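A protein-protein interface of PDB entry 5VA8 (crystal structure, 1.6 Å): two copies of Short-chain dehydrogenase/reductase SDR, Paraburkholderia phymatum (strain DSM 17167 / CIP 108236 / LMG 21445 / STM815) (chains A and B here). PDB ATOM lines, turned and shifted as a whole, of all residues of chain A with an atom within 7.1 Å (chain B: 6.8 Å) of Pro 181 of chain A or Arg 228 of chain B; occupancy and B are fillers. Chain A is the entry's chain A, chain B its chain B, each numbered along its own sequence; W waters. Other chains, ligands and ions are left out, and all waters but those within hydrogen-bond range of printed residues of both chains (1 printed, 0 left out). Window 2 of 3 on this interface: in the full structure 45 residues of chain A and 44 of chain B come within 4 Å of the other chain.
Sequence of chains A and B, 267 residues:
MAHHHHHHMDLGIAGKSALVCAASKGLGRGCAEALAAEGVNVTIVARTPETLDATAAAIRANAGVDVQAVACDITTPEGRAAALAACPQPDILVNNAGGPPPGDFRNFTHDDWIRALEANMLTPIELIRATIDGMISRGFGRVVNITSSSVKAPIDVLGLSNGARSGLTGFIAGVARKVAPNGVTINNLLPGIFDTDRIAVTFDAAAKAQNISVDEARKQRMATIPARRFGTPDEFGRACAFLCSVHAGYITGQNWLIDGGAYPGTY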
ATOM      1  N   GLY A 139      13.520  18.745 -14.344  1.00  0.00           N
ATOM      2  CA  GLY A 139      12.132  18.591 -13.963  1.00  0.00           C
ATOM      3  C   GLY A 139      11.140  19.106 -14.976  1.00  0.00           C
ATOM      4  O   GLY A 139       9.990  19.365 -14.624  1.00  0.00           O
ATOM      5  N   VAL A 175       8.249   4.456 -22.705  1.00  0.00           N
ATOM      6  CA  VAL A 175       9.148   5.473 -22.169  1.00  0.00           C
ATOM      7  C   VAL A 175       8.362   6.686 -21.667  1.00  0.00           C
ATOM      8  O   VAL A 175       8.732   7.298 -20.659  1.00  0.00           O
ATOM      9  CB  VAL A 175      10.225   5.857 -23.207  1.00  0.00           C
ATOM     10  CG1 VAL A 175       9.620   6.500 -24.435  1.00  0.00           C
ATOM     11  CG2 VAL A 175      11.265   6.784 -22.574  1.00  0.00           C
ATOM     12  N   ALA A 176       7.262   7.045 -22.339  1.00  0.00           N
ATOM     13  CA  ALA A 176       6.444   8.155 -21.841  1.00  0.00           C
ATOM     14  C   ALA A 176       6.031   7.913 -20.395  1.00  0.00           C
ATOM     15  O   ALA A 176       6.141   8.798 -19.538  1.00  0.00           O
ATOM     16  CB  ALA A 176       5.204   8.347 -22.721  1.00  0.00           C
ATOM     17  N   ARG A 177       5.576   6.708 -20.090  1.00  0.00           N
ATOM     18  CA  ARG A 177       5.109   6.493 -18.726  1.00  0.00           C
ATOM     19  C   ARG A 177       6.271   6.351 -17.748  1.00  0.00           C
ATOM     20  O   ARG A 177       6.134   6.715 -16.574  1.00  0.00           O
ATOM     21  CB  ARG A 177       4.170   5.292 -18.713  1.00  0.00           C
ATOM     22  CG  ARG A 177       2.829   5.661 -19.379  1.00  0.00           C
ATOM     23  CD  ARG A 177       2.145   4.480 -20.005  1.00  0.00           C
ATOM     24  NE  ARG A 177       0.830   4.818 -20.551  1.00  0.00           N
ATOM     25  CZ  ARG A 177       0.592   5.048 -21.839  1.00  0.00           C
ATOM     26  NH1 ARG A 177       1.585   5.005 -22.719  1.00  0.00           N
ATOM     27  NH2 ARG A 177      -0.636   5.317 -22.251  1.00  0.00           N
ATOM     28  N   LYS A 178       7.424   5.881 -18.227  1.00  0.00           N
ATOM     29  CA  LYS A 178       8.605   5.713 -17.382  1.00  0.00           C
ATOM     30  C   LYS A 178       9.134   7.053 -16.880  1.00  0.00           C
ATOM     31  O   LYS A 178       9.538   7.173 -15.712  1.00  0.00           O
ATOM     32  CB  LYS A 178       9.687   4.975 -18.179  1.00  0.00           C
ATOM     33  CG  LYS A 178      10.993   4.770 -17.431  1.00  0.00           C
ATOM     34  CD  LYS A 178      10.754   3.895 -16.218  1.00  0.00           C
ATOM     35  CE  LYS A 178      11.566   2.618 -16.288  1.00  0.00           C
ATOM     36  NZ  LYS A 178      11.281   1.757 -15.109  1.00  0.00           N
ATOM     37  N   VAL A 179       9.166   8.067 -17.750  1.00  0.00           N
ATOM     38  CA  VAL A 179       9.788   9.342 -17.412  1.00  0.00           C
ATOM     39  C   VAL A 179       8.785  10.366 -16.906  1.00  0.00           C
ATOM     40  O   VAL A 179       9.187  11.456 -16.465  1.00  0.00           O
ATOM     41  CB  VAL A 179      10.575   9.925 -18.607  1.00  0.00           C
ATOM     42  CG1 VAL A 179      11.623   8.932 -19.076  1.00  0.00           C
ATOM     43  CG2 VAL A 179       9.639  10.300 -19.756  1.00  0.00           C
ATOM     44  N   ALA A 180       7.496  10.040 -16.928  1.00  0.00           N
ATOM     45  CA  ALA A 180       6.486  10.993 -16.477  1.00  0.00           C
ATOM     46  C   ALA A 180       6.666  11.492 -15.042  1.00  0.00           C
ATOM     47  O   ALA A 180       6.247  12.635 -14.776  1.00  0.00           O
ATOM     48  CB  ALA A 180       5.084  10.378 -16.645  1.00  0.00           C
ATOM     49  N   PRO A 181       7.241  10.738 -14.094  1.00  0.00           N
ATOM     50  CA  PRO A 181       7.391  11.287 -12.735  1.00  0.00           C
ATOM     51  C   PRO A 181       8.261  12.526 -12.665  1.00  0.00           C
ATOM     52  O   PRO A 181       8.214  13.239 -11.651  1.00  0.00           O
ATOM     53  CB  PRO A 181       8.024  10.124 -11.958  1.00  0.00           C
ATOM     54  CG  PRO A 181       7.537   8.911 -12.658  1.00  0.00           C
ATOM     55  CD  PRO A 181       7.524   9.286 -14.108  1.00  0.00           C
ATOM     56  N   ASN A 182       9.049  12.801 -13.707  1.00  0.00           N
ATOM     57  CA  ASN A 182      10.062  13.850 -13.702  1.00  0.00           C
ATOM     58  C   ASN A 182       9.637  15.093 -14.475  1.00  0.00           C
ATOM     59  O   ASN A 182      10.492  15.891 -14.864  1.00  0.00           O
ATOM     60  CB  ASN A 182      11.366  13.305 -14.276  1.00  0.00           C
ATOM     61  CG  ASN A 182      11.779  12.017 -13.618  1.00  0.00           C
ATOM     62  OD1 ASN A 182      12.210  12.019 -12.466  1.00  0.00           O
ATOM     63  ND2 ASN A 182      11.644  10.901 -14.338  1.00  0.00           N
ATOM     64  N   GLY A 183       8.345  15.278 -14.707  1.00  0.00           N
ATOM     65  CA  GLY A 183       7.907  16.496 -15.359  1.00  0.00           C
ATOM     66  C   GLY A 183       8.142  16.517 -16.851  1.00  0.00           C
ATOM     67  O   GLY A 183       8.086  17.593 -17.461  1.00  0.00           O
ATOM     68  N   VAL A 184       8.408  15.361 -17.448  1.00  0.00           N
ATOM     69  CA  VAL A 184       8.630  15.219 -18.882  1.00  0.00           C
ATOM     70  C   VAL A 184       7.402  14.554 -19.482  1.00  0.00           C
ATOM     71  O   VAL A 184       6.873  13.586 -18.917  1.00  0.00           O
ATOM     72  CB  VAL A 184       9.890  14.382 -19.165  1.00  0.00           C
ATOM     73  CG1 VAL A 184      10.109  14.202 -20.665  1.00  0.00           C
ATOM     74  CG2 VAL A 184      11.096  15.031 -18.508  1.00  0.00           C
ATOM     75  N   TYR A 250      -0.123  17.332 -18.107  1.00  0.00           N
ATOM     76  CA  TYR A 250      -0.854  16.135 -17.706  1.00  0.00           C
ATOM     77  C   TYR A 250      -1.241  15.284 -18.909  1.00  0.00           C
ATOM     78  O   TYR A 250      -2.057  14.365 -18.774  1.00  0.00           O
ATOM     79  CB  TYR A 250      -2.102  16.510 -16.895  1.00  0.00           C
ATOM     80  CG  TYR A 250      -2.463  15.525 -15.806  1.00  0.00           C
ATOM     81  CD1 TYR A 250      -1.518  15.142 -14.854  1.00  0.00           C
ATOM     82  CD2 TYR A 250      -3.761  15.020 -15.689  1.00  0.00           C
ATOM     83  CE1 TYR A 250      -1.839  14.252 -13.831  1.00  0.00           C
ATOM     84  CE2 TYR A 250      -4.099  14.127 -14.667  1.00  0.00           C
ATOM     85  CZ  TYR A 250      -3.124  13.758 -13.736  1.00  0.00           C
ATOM     86  OH  TYR A 250      -3.454  12.882 -12.727  1.00  0.00           O
ATOM     87  N   ARG B 221      -2.639   7.979  -3.728  1.00  0.00           N
ATOM     88  CA  ARG B 221      -3.155   7.868  -5.087  1.00  0.00           C
ATOM     89  C   ARG B 221      -2.172   8.439  -6.103  1.00  0.00           C
ATOM     90  O   ARG B 221      -1.963   7.846  -7.168  1.00  0.00           O
ATOM     91  CB  ARG B 221      -4.509   8.574  -5.191  1.00  0.00           C
ATOM     92  CG  ARG B 221      -5.110   8.598  -6.599  1.00  0.00           C
ATOM     93  CD  ARG B 221      -5.407   7.188  -7.104  1.00  0.00           C
ATOM     94  NE  ARG B 221      -5.766   7.210  -8.523  1.00  0.00           N
ATOM     95  CZ  ARG B 221      -6.996   7.432  -8.970  1.00  0.00           C
ATOM     96  NH1 ARG B 221      -7.992   7.635  -8.112  1.00  0.00           N
ATOM     97  NH2 ARG B 221      -7.232   7.449 -10.276  1.00  0.00           N
ATOM     98  N   MET B 222      -1.564   9.594  -5.798  1.00  0.00           N
ATOM     99  CA  MET B 222      -0.622  10.207  -6.734  1.00  0.00           C
ATOM    100  C   MET B 222       0.539   9.281  -7.055  1.00  0.00           C
ATOM    101  O   MET B 222       1.071   9.319  -8.173  1.00  0.00           O
ATOM    102  CB  MET B 222      -0.072  11.517  -6.174  1.00  0.00           C
ATOM    103  CG  MET B 222      -1.082  12.623  -6.037  1.00  0.00           C
ATOM    104  SD  MET B 222      -0.320  14.130  -5.432  1.00  0.00           S
ATOM    105  CE  MET B 222      -1.761  14.958  -4.759  1.00  0.00           C
ATOM    106  N   ALA B 223       0.955   8.460  -6.087  1.00  0.00           N
ATOM    107  CA  ALA B 223       2.099   7.579  -6.281  1.00  0.00           C
ATOM    108  C   ALA B 223       1.860   6.551  -7.378  1.00  0.00           C
ATOM    109  O   ALA B 223       2.826   6.015  -7.930  1.00  0.00           O
ATOM    110  CB  ALA B 223       2.439   6.871  -4.968  1.00  0.00           C
ATOM    111  N   THR B 224       0.603   6.266  -7.704  1.00  0.00           N
ATOM    112  CA  THR B 224       0.257   5.320  -8.755  1.00  0.00           C
ATOM    113  C   THR B 224       0.103   5.970 -10.127  1.00  0.00           C
ATOM    114  O   THR B 224      -0.050   5.252 -11.119  1.00  0.00           O
ATOM    115  CB  THR B 224      -1.044   4.598  -8.402  1.00  0.00           C
ATOM    116  OG1 THR B 224      -2.145   5.504  -8.556  1.00  0.00           O
ATOM    117  CG2 THR B 224      -0.998   4.107  -6.953  1.00  0.00           C
ATOM    118  N   ILE B 225       0.132   7.290 -10.215  1.00  0.00           N
ATOM    119  CA  ILE B 225      -0.053   8.006 -11.477  1.00  0.00           C
ATOM    120  C   ILE B 225       1.327   8.327 -12.033  1.00  0.00           C
ATOM    121  O   ILE B 225       2.159   8.867 -11.297  1.00  0.00           O
ATOM    122  CB  ILE B 225      -0.866   9.294 -11.273  1.00  0.00           C
ATOM    123  CG1 ILE B 225      -2.229   8.959 -10.673  1.00  0.00           C
ATOM    124  CG2 ILE B 225      -1.011  10.063 -12.590  1.00  0.00           C
ATOM    125  CD1 ILE B 225      -2.951  10.175 -10.196  1.00  0.00           C
ATOM    126  N   PRO B 226       1.621   8.007 -13.298  1.00  0.00           N
ATOM    127  CA  PRO B 226       2.983   8.281 -13.792  1.00  0.00           C
ATOM    128  C   PRO B 226       3.407   9.735 -13.613  1.00  0.00           C
ATOM    129  O   PRO B 226       4.543   9.981 -13.196  1.00  0.00           O
ATOM    130  CB  PRO B 226       2.904   7.855 -15.260  1.00  0.00           C
ATOM    131  CG  PRO B 226       1.891   6.729 -15.234  1.00  0.00           C
ATOM    132  CD  PRO B 226       0.828   7.248 -14.285  1.00  0.00           C
ATOM    133  N   ALA B 227       2.518  10.701 -13.845  1.00  0.00           N
ATOM    134  CA  ALA B 227       2.872  12.099 -13.609  1.00  0.00           C
ATOM    135  C   ALA B 227       3.003  12.452 -12.128  1.00  0.00           C
ATOM    136  O   ALA B 227       3.518  13.536 -11.821  1.00  0.00           O
ATOM    137  CB  ALA B 227       1.836  13.029 -14.253  1.00  0.00           C
ATOM    138  N   ARG B 228       2.533  11.593 -11.216  1.00  0.00           N
ATOM    139  CA  ARG B 228       2.709  11.757  -9.766  1.00  0.00           C
ATOM    140  C   ARG B 228       1.976  12.978  -9.212  1.00  0.00           C
ATOM    141  O   ARG B 228       2.382  13.551  -8.193  1.00  0.00           O
ATOM    142  CB  ARG B 228       4.194  11.813  -9.399  1.00  0.00           C
ATOM    143  CG  ARG B 228       4.971  10.561  -9.767  1.00  0.00           C
ATOM    144  CD  ARG B 228       4.618   9.391  -8.869  1.00  0.00           C
ATOM    145  NE  ARG B 228       5.604   8.322  -9.019  1.00  0.00           N
ATOM    146  CZ  ARG B 228       5.479   7.307  -9.865  1.00  0.00           C
ATOM    147  NH1 ARG B 228       4.398   7.200 -10.622  1.00  0.00           N
ATOM    148  NH2 ARG B 228       6.431   6.390  -9.946  1.00  0.00           N
ATOM    149  N   ARG B 229       0.885  13.378  -9.862  1.00  0.00           N
ATOM    150  CA  ARG B 229       0.049  14.468  -9.386  1.00  0.00           C
ATOM    151  C   ARG B 229      -1.353  14.258  -9.937  1.00  0.00           C
ATOM    152  O   ARG B 229      -1.577  13.398 -10.796  1.00  0.00           O
ATOM    153  CB  ARG B 229       0.603  15.829  -9.818  1.00  0.00           C
ATOM    154  CG  ARG B 229       0.625  16.066 -11.332  1.00  0.00           C
ATOM    155  CD  ARG B 229       0.940  17.521 -11.568  1.00  0.00           C
ATOM    156  NE  ARG B 229       1.101  17.946 -12.967  1.00  0.00           N
ATOM    157  CZ  ARG B 229       0.096  18.360 -13.734  1.00  0.00           C
ATOM    158  NH1 ARG B 229      -1.158  18.351 -13.275  1.00  0.00           N
ATOM    159  NH2 ARG B 229       0.346  18.780 -14.969  1.00  0.00           N
ATOM    160  N   PHE B 230      -2.295  15.059  -9.437  1.00  0.00           N
ATOM    161  CA  PHE B 230      -3.628  15.141 -10.024  1.00  0.00           C
ATOM    162  C   PHE B 230      -3.655  16.246 -11.071  1.00  0.00           C
ATOM    163  O   PHE B 230      -2.820  17.150 -11.076  1.00  0.00           O
ATOM    164  CB  PHE B 230      -4.704  15.433  -8.972  1.00  0.00           C
ATOM    165  CG  PHE B 230      -4.793  14.419  -7.861  1.00  0.00           C
ATOM    166  CD1 PHE B 230      -4.372  13.112  -8.033  1.00  0.00           C
ATOM    167  CD2 PHE B 230      -5.319  14.790  -6.630  1.00  0.00           C
ATOM    168  CE1 PHE B 230      -4.469  12.198  -6.993  1.00  0.00           C
ATOM    169  CE2 PHE B 230      -5.419  13.875  -5.584  1.00  0.00           C
ATOM    170  CZ  PHE B 230      -4.992  12.583  -5.767  1.00  0.00           C
ATOM    171  N   GLY B 260      -2.178  12.187 -17.092  1.00  0.00           N
ATOM    172  CA  GLY B 260      -0.846  11.972 -16.552  1.00  0.00           C
ATOM    173  C   GLY B 260      -0.267  10.609 -16.842  1.00  0.00           C
ATOM    174  O   GLY B 260       0.606  10.142 -16.110  1.00  0.00           O
HETATM  175  O   HOH W   1       5.587  15.096 -13.187  1.00  0.00           O
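N of Gly 260 of chain B sits at hydrogen-bond distance from O of Tyr 250 of chain A (2.8 Å).
N of Pro 181 of chain A lies close to O of Pro 226 of chain B, at 2.9 Å.
The side-chain hydroxyl (OH) of Tyr 250 of chain A is in hydrogen-bond range of the backbone carbonyl oxygen (O) of Arg 229 of chain B, 2.7 Å away.
NH1 of Arg 228 of chain B lies within hydrogen-bond range of O of Ala 223 of chain B, at 3.3 Å.
NH1 of Arg 228 of chain B sits at hydrogen-bond distance from O of Ile 225 of chain B (2.9 Å).
The backbone carbonyl oxygen (O) of Gly 260 of chain B lies within hydrogen-bond range of the backbone NH (N) of Ala 227 of chain B (3.0 Å).
CB of Pro 226 of chain B touches O of Arg 177 of chain A, 3.7 Å away.
Pro 226 of chain B touches Ala 180 of chain A.
Ala 227 of chain B touches Ala 180 of chain A (CA to O, 3.6 Å).
Pro 181 of chain A touches Arg 228 of chain B.
Tyr 250 of chain A touches Ile 225 of chain B (OH to CG2, 3.7 Å).
CE1 of Tyr 250 of chain A touches CB of Ala 227 of chain B, at 3.9 Å.
OH of Tyr 250 of chain A touches CA of Phe 230 of chain B, 3.5 Å away.
Of chain B, only Pro 226 (2.9 Å) and Arg 228 (3.8 Å) come within 4 Å of Pro 181 of chain A.
Arg 228 of chain B touches just one residue of chain A: Pro 181 (3.8 Å).
Of the printed residues of chain A, Ala 227 of chain B touches Ala 180 and Tyr 250.
Of the printed residues of chain A, Pro 226 of chain B touches Arg 177 (3.7 Å), Ala 180 (3.2 Å) and Pro 181 (2.9 Å).
Arg 221 of chain B touches none of the printed residues of chain A.
Ala 223 of chain B touches none of the printed residues of chain A.
The nearest printed residue of chain B that does not touch Arg 177 of chain A is Gly 260 of chain B (6.0 Å).
Hydrophobic or aromatic side chains of chain B within 4 Å of the printed part of chain A: Ile 225, Pro 226 and Ala 227.
Printed residues of chain A that touch a printed residue of chain B: Arg 177, Ala 180, Pro 181 and Tyr 250.
Hydrophobic or aromatic side chains of chain A that line the printed part of chain B: Ala 180, Pro 181 and Tyr 250.
Among the printed residues, 10 pairs touch across the chains.
No position is printed for both chains.
Of the 10 pairs that touch across the chains among the printed residues, none has its exchanged pair printed and touching as well.
Water W1 lies within hydrogen-bond range of the backbone carbonyl oxygen of Ala 227 of chain B (2.9 Å), the backbone carbonyl oxygen of Ala 180 of chain A (3.0 Å) and the backbone NH of Gly 183 of chain A (3.2 Å).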
